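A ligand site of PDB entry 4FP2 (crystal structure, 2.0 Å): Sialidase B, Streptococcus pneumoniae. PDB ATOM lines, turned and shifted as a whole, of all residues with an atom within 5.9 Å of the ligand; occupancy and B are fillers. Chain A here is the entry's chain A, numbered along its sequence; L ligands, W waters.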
ATOM      1  N   ARG A 245      13.516  15.418   7.194  1.00  0.00           N
ATOM      2  CA  ARG A 245      12.545  15.770   6.170  1.00  0.00           C
ATOM      3  C   ARG A 245      13.257  16.260   4.904  1.00  0.00           C
ATOM      4  O   ARG A 245      14.457  16.543   4.911  1.00  0.00           O
ATOM      5  CB  ARG A 245      11.580  16.857   6.685  1.00  0.00           C
ATOM      6  CG  ARG A 245      10.401  16.329   7.550  1.00  0.00           C
ATOM      7  CD  ARG A 245       9.164  17.275   7.449  1.00  0.00           C
ATOM      8  NE  ARG A 245       8.706  17.398   6.062  1.00  0.00           N
ATOM      9  CZ  ARG A 245       7.792  18.261   5.624  1.00  0.00           C
ATOM     10  NH1 ARG A 245       7.190  19.102   6.466  1.00  0.00           N
ATOM     11  NH2 ARG A 245       7.469  18.270   4.331  1.00  0.00           N
ATOM     12  N   ILE A 246      12.492  16.390   3.814  1.00  0.00           N
ATOM     13  CA  ILE A 246      12.950  17.050   2.592  1.00  0.00           C
ATOM     14  C   ILE A 246      14.149  16.350   1.955  1.00  0.00           C
ATOM     15  O   ILE A 246      15.240  16.914   1.926  1.00  0.00           O
ATOM     16  CB  ILE A 246      13.331  18.542   2.815  1.00  0.00           C
ATOM     17  CG1 ILE A 246      12.444  19.221   3.870  1.00  0.00           C
ATOM     18  CG2 ILE A 246      13.263  19.287   1.514  1.00  0.00           C
ATOM     19  CD1 ILE A 246      10.945  19.283   3.508  1.00  0.00           C
ATOM     20  N   ARG A 264      16.532  17.366  11.189  1.00  0.00           N
ATOM     21  CA  ARG A 264      15.729  18.218  12.054  1.00  0.00           C
ATOM     22  C   ARG A 264      15.760  17.728  13.502  1.00  0.00           C
ATOM     23  O   ARG A 264      15.385  16.599  13.808  1.00  0.00           O
ATOM     24  CB  ARG A 264      14.290  18.350  11.544  1.00  0.00           C
ATOM     25  CG  ARG A 264      14.188  18.882  10.103  1.00  0.00           C
ATOM     26  CD  ARG A 264      12.761  19.227   9.704  1.00  0.00           C
ATOM     27  NE  ARG A 264      12.737  19.913   8.407  1.00  0.00           N
ATOM     28  CZ  ARG A 264      11.651  20.464   7.852  1.00  0.00           C
ATOM     29  NH1 ARG A 264      10.466  20.442   8.472  1.00  0.00           N
ATOM     30  NH2 ARG A 264      11.756  21.058   6.669  1.00  0.00           N
ATOM     31  N   ASP A 270       9.113  22.630  10.562  1.00  0.00           N
ATOM     32  CA  ASP A 270       9.825  23.618   9.759  1.00  0.00           C
ATOM     33  C   ASP A 270      10.479  24.642  10.696  1.00  0.00           C
ATOM     34  O   ASP A 270      10.048  24.792  11.842  1.00  0.00           O
ATOM     35  CB  ASP A 270       8.852  24.376   8.831  1.00  0.00           C
ATOM     36  CG  ASP A 270       8.415  23.576   7.611  1.00  0.00           C
ATOM     37  OD1 ASP A 270       7.700  24.170   6.766  1.00  0.00           O
ATOM     38  OD2 ASP A 270       8.771  22.388   7.465  1.00  0.00           O
ATOM     39  N   ILE A 326      17.330  24.951   5.797  1.00  0.00           N
ATOM     40  CA  ILE A 326      16.118  24.227   5.433  1.00  0.00           C
ATOM     41  C   ILE A 326      15.921  24.237   3.919  1.00  0.00           C
ATOM     42  O   ILE A 326      16.199  25.241   3.265  1.00  0.00           O
ATOM     43  CB  ILE A 326      14.869  24.795   6.204  1.00  0.00           C
ATOM     44  CG1 ILE A 326      13.571  24.072   5.834  1.00  0.00           C
ATOM     45  CG2 ILE A 326      14.736  26.312   6.039  1.00  0.00           C
ATOM     46  CD1 ILE A 326      12.415  24.447   6.787  1.00  0.00           C
ATOM     47  N   ASP A 327      15.495  23.087   3.382  1.00  0.00           N
ATOM     48  CA  ASP A 327      15.214  22.894   1.950  1.00  0.00           C
ATOM     49  C   ASP A 327      16.487  22.948   1.095  1.00  0.00           C
ATOM     50  O   ASP A 327      16.830  24.001   0.569  1.00  0.00           O
ATOM     51  CB  ASP A 327      14.208  23.902   1.395  1.00  0.00           C
ATOM     52  CG  ASP A 327      12.809  23.720   1.951  1.00  0.00           C
ATOM     53  OD1 ASP A 327      12.559  22.693   2.586  1.00  0.00           O
ATOM     54  OD2 ASP A 327      11.951  24.606   1.712  1.00  0.00           O
ATOM     55  N   ASP A 344      18.093  27.143   1.999  1.00  0.00           N
ATOM     56  CA  ASP A 344      17.678  28.360   2.706  1.00  0.00           C
ATOM     57  C   ASP A 344      18.421  28.466   4.034  1.00  0.00           C
ATOM     58  O   ASP A 344      18.700  27.447   4.697  1.00  0.00           O
ATOM     59  CB  ASP A 344      16.166  28.386   3.012  1.00  0.00           C
ATOM     60  CG  ASP A 344      15.288  28.252   1.771  1.00  0.00           C
ATOM     61  OD1 ASP A 344      15.720  28.582   0.641  1.00  0.00           O
ATOM     62  OD2 ASP A 344      14.132  27.822   1.944  1.00  0.00           O
ATOM     63  N   MET A 346      18.197  30.442   7.837  1.00  0.00           N
ATOM     64  CA  MET A 346      17.353  31.188   8.766  1.00  0.00           C
ATOM     65  C   MET A 346      18.181  31.586   9.986  1.00  0.00           C
ATOM     66  O   MET A 346      18.726  30.721  10.669  1.00  0.00           O
ATOM     67  CB  MET A 346      16.199  30.303   9.257  1.00  0.00           C
ATOM     68  CG  MET A 346      15.271  29.804   8.184  1.00  0.00           C
ATOM     69  SD  MET A 346      14.275  31.108   7.450  1.00  0.00           S
ATOM     70  CE  MET A 346      13.431  30.161   6.179  1.00  0.00           C
ATOM     71  N   GLY A 351      11.754  31.735  10.836  1.00  0.00           N
ATOM     72  CA  GLY A 351      11.234  30.786   9.867  1.00  0.00           C
ATOM     73  C   GLY A 351      10.428  31.589   8.855  1.00  0.00           C
ATOM     74  O   GLY A 351      10.486  32.820   8.877  1.00  0.00           O
ATOM     75  N   ASN A 352       9.700  30.912   7.970  1.00  0.00           N
ATOM     76  CA  ASN A 352       8.857  31.612   6.998  1.00  0.00           C
ATOM     77  C   ASN A 352       7.874  32.569   7.664  1.00  0.00           C
ATOM     78  O   ASN A 352       7.684  33.697   7.200  1.00  0.00           O
ATOM     79  CB  ASN A 352       8.088  30.617   6.120  1.00  0.00           C
ATOM     80  CG  ASN A 352       6.840  31.228   5.501  1.00  0.00           C
ATOM     81  OD1 ASN A 352       6.930  32.033   4.575  1.00  0.00           O
ATOM     82  ND2 ASN A 352       5.674  30.855   6.021  1.00  0.00           N
ATOM     83  N   TYR A 489      12.511  31.477  -2.020  1.00  0.00           N
ATOM     84  CA  TYR A 489      12.605  30.204  -1.314  1.00  0.00           C
ATOM     85  C   TYR A 489      13.084  29.122  -2.273  1.00  0.00           C
ATOM     86  O   TYR A 489      12.449  28.872  -3.294  1.00  0.00           O
ATOM     87  CB  TYR A 489      11.255  29.822  -0.733  1.00  0.00           C
ATOM     88  CG  TYR A 489      10.685  30.864   0.198  1.00  0.00           C
ATOM     89  CD1 TYR A 489      11.362  31.230   1.352  1.00  0.00           C
ATOM     90  CD2 TYR A 489       9.464  31.460  -0.069  1.00  0.00           C
ATOM     91  CE1 TYR A 489      10.845  32.176   2.213  1.00  0.00           C
ATOM     92  CE2 TYR A 489       8.939  32.417   0.787  1.00  0.00           C
ATOM     93  CZ  TYR A 489       9.627  32.768   1.929  1.00  0.00           C
ATOM     94  OH  TYR A 489       9.099  33.702   2.778  1.00  0.00           O
ATOM     95  N   TYR A 509      11.067  30.005  -5.540  1.00  0.00           N
ATOM     96  CA  TYR A 509       9.767  30.660  -5.691  1.00  0.00           C
ATOM     97  C   TYR A 509       9.593  31.800  -4.701  1.00  0.00           C
ATOM     98  O   TYR A 509      10.291  31.896  -3.682  1.00  0.00           O
ATOM     99  CB  TYR A 509       8.602  29.664  -5.557  1.00  0.00           C
ATOM    100  CG  TYR A 509       8.485  29.047  -4.166  1.00  0.00           C
ATOM    101  CD1 TYR A 509       7.655  29.619  -3.190  1.00  0.00           C
ATOM    102  CD2 TYR A 509       9.222  27.927  -3.809  1.00  0.00           C
ATOM    103  CE1 TYR A 509       7.550  29.062  -1.906  1.00  0.00           C
ATOM    104  CE2 TYR A 509       9.133  27.368  -2.539  1.00  0.00           C
ATOM    105  CZ  TYR A 509       8.293  27.941  -1.590  1.00  0.00           C
ATOM    106  OH  TYR A 509       8.222  27.380  -0.334  1.00  0.00           O
ATOM    107  N   THR A 539       3.142  27.955  -2.090  1.00  0.00           N
ATOM    108  CA  THR A 539       4.371  27.214  -1.886  1.00  0.00           C
ATOM    109  C   THR A 539       4.613  26.510  -3.206  1.00  0.00           C
ATOM    110  O   THR A 539       4.211  25.363  -3.389  1.00  0.00           O
ATOM    111  CB  THR A 539       4.191  26.219  -0.731  1.00  0.00           C
ATOM    112  OG1 THR A 539       3.792  26.939   0.445  1.00  0.00           O
ATOM    113  CG2 THR A 539       5.500  25.469  -0.436  1.00  0.00           C
ATOM    114  N   GLU A 541       6.779  24.826  -5.019  1.00  0.00           N
ATOM    115  CA  GLU A 541       7.984  24.019  -5.118  1.00  0.00           C
ATOM    116  C   GLU A 541       8.032  23.375  -6.491  1.00  0.00           C
ATOM    117  O   GLU A 541       7.104  22.665  -6.879  1.00  0.00           O
ATOM    118  CB  GLU A 541       8.010  22.987  -3.998  1.00  0.00           C
ATOM    119  CG  GLU A 541       8.155  23.622  -2.608  1.00  0.00           C
ATOM    120  CD  GLU A 541       7.644  22.731  -1.489  1.00  0.00           C
ATOM    121  OE1 GLU A 541       8.102  22.884  -0.338  1.00  0.00           O
ATOM    122  OE2 GLU A 541       6.769  21.887  -1.752  1.00  0.00           O
ATOM    123  N   ARG A 557       4.172  22.522  -7.543  1.00  0.00           N
ATOM    124  CA  ARG A 557       3.096  22.455  -6.565  1.00  0.00           C
ATOM    125  C   ARG A 557       2.286  23.754  -6.591  1.00  0.00           C
ATOM    126  O   ARG A 557       2.842  24.834  -6.741  1.00  0.00           O
ATOM    127  CB  ARG A 557       3.711  22.244  -5.181  1.00  0.00           C
ATOM    128  CG  ARG A 557       2.802  22.475  -3.965  1.00  0.00           C
ATOM    129  CD  ARG A 557       3.622  22.327  -2.685  1.00  0.00           C
ATOM    130  NE  ARG A 557       2.843  22.638  -1.484  1.00  0.00           N
ATOM    131  CZ  ARG A 557       3.279  22.451  -0.250  1.00  0.00           C
ATOM    132  NH1 ARG A 557       4.506  21.952  -0.003  1.00  0.00           N
ATOM    133  NH2 ARG A 557       2.469  22.759   0.759  1.00  0.00           N
ATOM    134  N   TYR A 589      -3.569  22.257  -0.423  1.00  0.00           N
ATOM    135  CA  TYR A 589      -2.273  22.836  -0.022  1.00  0.00           C
ATOM    136  C   TYR A 589      -1.093  22.304  -0.832  1.00  0.00           C
ATOM    137  O   TYR A 589      -0.045  22.944  -0.917  1.00  0.00           O
ATOM    138  CB  TYR A 589      -2.020  22.650   1.470  1.00  0.00           C
ATOM    139  CG  TYR A 589      -2.201  21.226   1.954  1.00  0.00           C
ATOM    140  CD1 TYR A 589      -1.149  20.325   1.923  1.00  0.00           C
ATOM    141  CD2 TYR A 589      -3.426  20.789   2.441  1.00  0.00           C
ATOM    142  CE1 TYR A 589      -1.308  19.026   2.359  1.00  0.00           C
ATOM    143  CE2 TYR A 589      -3.597  19.498   2.897  1.00  0.00           C
ATOM    144  CZ  TYR A 589      -2.534  18.620   2.832  1.00  0.00           C
ATOM    145  OH  TYR A 589      -2.688  17.334   3.267  1.00  0.00           O
ATOM    146  N   GLY A 590      -1.260  21.121  -1.424  1.00  0.00           N
ATOM    147  CA  GLY A 590      -0.251  20.591  -2.337  1.00  0.00           C
ATOM    148  C   GLY A 590       0.904  19.917  -1.632  1.00  0.00           C
ATOM    149  O   GLY A 590       0.983  19.926  -0.406  1.00  0.00           O
ATOM    150  N   ARG A 619      -1.539  13.463   2.262  1.00  0.00           N
ATOM    151  CA  ARG A 619      -0.268  13.113   1.623  1.00  0.00           C
ATOM    152  C   ARG A 619      -0.116  11.615   1.751  1.00  0.00           C
ATOM    153  O   ARG A 619       0.451  11.112   2.708  1.00  0.00           O
ATOM    154  CB  ARG A 619       0.899  13.891   2.249  1.00  0.00           C
ATOM    155  CG  ARG A 619       0.846  15.375   1.939  1.00  0.00           C
ATOM    156  CD  ARG A 619       1.963  16.175   2.623  1.00  0.00           C
ATOM    157  NE  ARG A 619       2.105  17.500   2.020  1.00  0.00           N
ATOM    158  CZ  ARG A 619       2.919  18.451   2.470  1.00  0.00           C
ATOM    159  NH1 ARG A 619       3.666  18.242   3.555  1.00  0.00           N
ATOM    160  NH2 ARG A 619       2.975  19.618   1.854  1.00  0.00           N
ATOM    161  N   TYR A 653       6.908  14.458   0.630  1.00  0.00           N
ATOM    162  CA  TYR A 653       8.048  14.936  -0.147  1.00  0.00           C
ATOM    163  C   TYR A 653       8.878  13.758  -0.645  1.00  0.00           C
ATOM    164  O   TYR A 653       9.003  12.727   0.037  1.00  0.00           O
ATOM    165  CB  TYR A 653       8.928  15.895   0.664  1.00  0.00           C
ATOM    166  CG  TYR A 653       8.385  17.320   0.755  1.00  0.00           C
ATOM    167  CD1 TYR A 653       7.041  17.569   1.017  1.00  0.00           C
ATOM    168  CD2 TYR A 653       9.230  18.407   0.602  1.00  0.00           C
ATOM    169  CE1 TYR A 653       6.551  18.867   1.105  1.00  0.00           C
ATOM    170  CE2 TYR A 653       8.756  19.723   0.708  1.00  0.00           C
ATOM    171  CZ  TYR A 653       7.418  19.945   0.959  1.00  0.00           C
ATOM    172  OH  TYR A 653       6.936  21.232   1.051  1.00  0.00           O
ATOM    173  N   GLU A 669       9.498  10.742   2.093  1.00  0.00           N
ATOM    174  CA  GLU A 669       8.775  10.814   3.352  1.00  0.00           C
ATOM    175  C   GLU A 669       7.617   9.811   3.332  1.00  0.00           C
ATOM    176  O   GLU A 669       6.586  10.051   2.689  1.00  0.00           O
ATOM    177  CB  GLU A 669       8.251  12.250   3.536  1.00  0.00           C
ATOM    178  CG  GLU A 669       9.363  13.298   3.620  1.00  0.00           C
ATOM    179  CD  GLU A 669       8.863  14.718   3.885  1.00  0.00           C
ATOM    180  OE1 GLU A 669       7.644  14.944   3.743  1.00  0.00           O
ATOM    181  OE2 GLU A 669       9.699  15.595   4.217  1.00  0.00           O
ATOM    182  N   SER A 673       3.270  14.301   5.989  1.00  0.00           N
ATOM    183  CA  SER A 673       4.077  15.312   6.641  1.00  0.00           C
ATOM    184  C   SER A 673       3.327  16.644   6.783  1.00  0.00           C
ATOM    185  O   SER A 673       3.898  17.636   7.229  1.00  0.00           O
ATOM    186  CB  SER A 673       5.400  15.484   5.908  1.00  0.00           C
ATOM    187  OG  SER A 673       5.212  16.041   4.606  1.00  0.00           O
ATOM    188  N   TRP A 674       2.055  16.652   6.401  1.00  0.00           N
ATOM    189  CA  TRP A 674       1.156  17.779   6.673  1.00  0.00           C
ATOM    190  C   TRP A 674       0.350  17.528   7.933  1.00  0.00           C
ATOM    191  O   TRP A 674       0.125  18.441   8.728  1.00  0.00           O
ATOM    192  CB  TRP A 674       0.226  18.036   5.485  1.00  0.00           C
ATOM    193  CG  TRP A 674      -0.581  19.324   5.572  1.00  0.00           C
ATOM    194  CD1 TRP A 674      -1.875  19.459   6.043  1.00  0.00           C
ATOM    195  CD2 TRP A 674      -0.170  20.637   5.177  1.00  0.00           C
ATOM    196  NE1 TRP A 674      -2.265  20.784   5.959  1.00  0.00           N
ATOM    197  CE2 TRP A 674      -1.251  21.524   5.423  1.00  0.00           C
ATOM    198  CE3 TRP A 674       1.020  21.153   4.624  1.00  0.00           C
ATOM    199  CZ2 TRP A 674      -1.167  22.888   5.162  1.00  0.00           C
ATOM    200  CZ3 TRP A 674       1.086  22.515   4.347  1.00  0.00           C
ATOM    201  CH2 TRP A 674       0.006  23.364   4.614  1.00  0.00           C
HETATM  202  C1  LIG L   1      10.183  26.203   4.362  1.00  0.00           C
HETATM  203  C2  LIG L   1      11.514  26.855   4.103  1.00  0.00           C
HETATM  204  C3  LIG L   1      11.407  28.229   3.529  1.00  0.00           C
HETATM  205  C4  LIG L   1      10.116  28.898   3.889  1.00  0.00           C
HETATM  206  C5  LIG L   1       8.933  28.138   3.345  1.00  0.00           C
HETATM  207  C6  LIG L   1       9.118  26.647   3.401  1.00  0.00           C
HETATM  208  C7  LIG L   1       7.824  25.940   3.733  1.00  0.00           C
HETATM  209  N1  LIG L   1       7.978  24.561   4.131  1.00  0.00           N
HETATM  210  C8  LIG L   1       6.777  23.789   3.737  1.00  0.00           C
HETATM  211  C9  LIG L   1       6.767  22.309   4.154  1.00  0.00           C
HETATM  212  S1  LIG L   1       5.175  21.574   4.228  1.00  0.00           S
HETATM  213  O1  LIG L   1       4.448  22.171   5.340  1.00  0.00           O
HETATM  214  O2  LIG L   1       5.338  20.131   4.460  1.00  0.00           O
HETATM  215  O3  LIG L   1       4.385  21.826   2.949  1.00  0.00           O
HETATM  216  O   HOH W   1      10.331  22.585   4.344  1.00  0.00           O
HETATM  217  O   HOH W   2       9.552  23.031   2.042  1.00  0.00           O
HETATM  218  O   HOH W   3       3.869  20.403   7.592  1.00  0.00           O
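The side-chain carboxylate of Asp 270 lies within salt-bridge range of a nitrogen (N1) of the ligand (2.7 Å). The guanidinium group of Arg 619 lies within salt-bridge range of an oxygen (O2) of the ligand, at 2.7 Å. The guanidinium group (NH2) of Arg 245 is in salt-bridge range of an oxygen (O2) of the ligand. NH1 of Arg 557 is in salt-bridge range of O3 of the ligand. An oxygen (O3) of the ligand sits at hydrogen-bond distance from the side-chain hydroxyl (OH) of Tyr 653, 3.2 Å away.
The guanidinium group (NH1) of Arg 619 is in hydrogen-bond range of the side-chain hydroxyl (OG) of Ser 673 (2.9 Å). The guanidinium group (NE) of Arg 245 is in salt-bridge range of the side-chain carboxylate (OE2) of Glu 669, at 2.8 Å. The backbone carbonyl oxygen of Gly 590 is in hydrogen-bond range of the guanidinium group of Arg 557. The backbone carbonyl oxygen (O) of Tyr 589 lies within hydrogen-bond range of the guanidinium group (NE) of Arg 557. The backbone carbonyl oxygen of Ile 326 is in hydrogen-bond range of the backbone NH of Asp 344 (3.0 Å). The side-chain hydroxyl (OH) of Tyr 489 lies within hydrogen-bond range of the side-chain amide oxygen (OD1) of Asn 352, at 3.3 Å. The backbone NH of Tyr 489 sits at hydrogen-bond distance from the backbone carbonyl oxygen of Tyr 509, 2.8 Å away. The side-chain hydroxyl (OG) of Ser 673 is in hydrogen-bond range of the side-chain carboxylate (OE1) of Glu 669 (2.8 Å).
Ile 326 touches the ligand (CD1 to C2, 3.7 Å). OD2 of Asp 327 touches C2 of the ligand, at 3.3 Å. Asp 344 touches the ligand (OD2 to C3, 3.2 Å). Met 346 touches the ligand (CE to C3, 3.9 Å). CB of Asn 352 touches C4 of the ligand, at 3.5 Å. CD1 of Tyr 489 touches C4 of the ligand (3.7 Å). Tyr 509 touches the ligand (OH to C5, 3.8 Å). O of Ser 673 touches O2 of the ligand, 3.996 Å away. Trp 674 touches the ligand (CZ3 to O1, 3.5 Å). Hydrophobic or aromatic side chains that line the ligand: Ile 326, Met 346, Tyr 489, Tyr 653 and Trp 674. Within 4 Å of the ligand: Arg 245, Asp 270, Ile 326, Asp 327, Asp 344, Met 346, Asn 352, Tyr 489, Tyr 509, Arg 557, Arg 619, Tyr 653, Ser 673 and Trp 674.
Water W3 bridges the backbone carbonyl oxygen of Ser 673 (2.8 Å) and an oxygen (O1) of the ligand (2.9 Å). Water W2 lies within hydrogen-bond range of the side-chain carboxylate of Glu 541, the side-chain carboxylate of Asp 327, a nitrogen (N1) of the ligand and the side-chain hydroxyl of Tyr 653. Water W1 lies within hydrogen-bond range of OD1 of Asp 327 (2.8 Å), N1 of the ligand (3.1 Å), NH2 of Arg 264 (3.1 Å) and OD2 of Asp 270 (3.5 Å).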
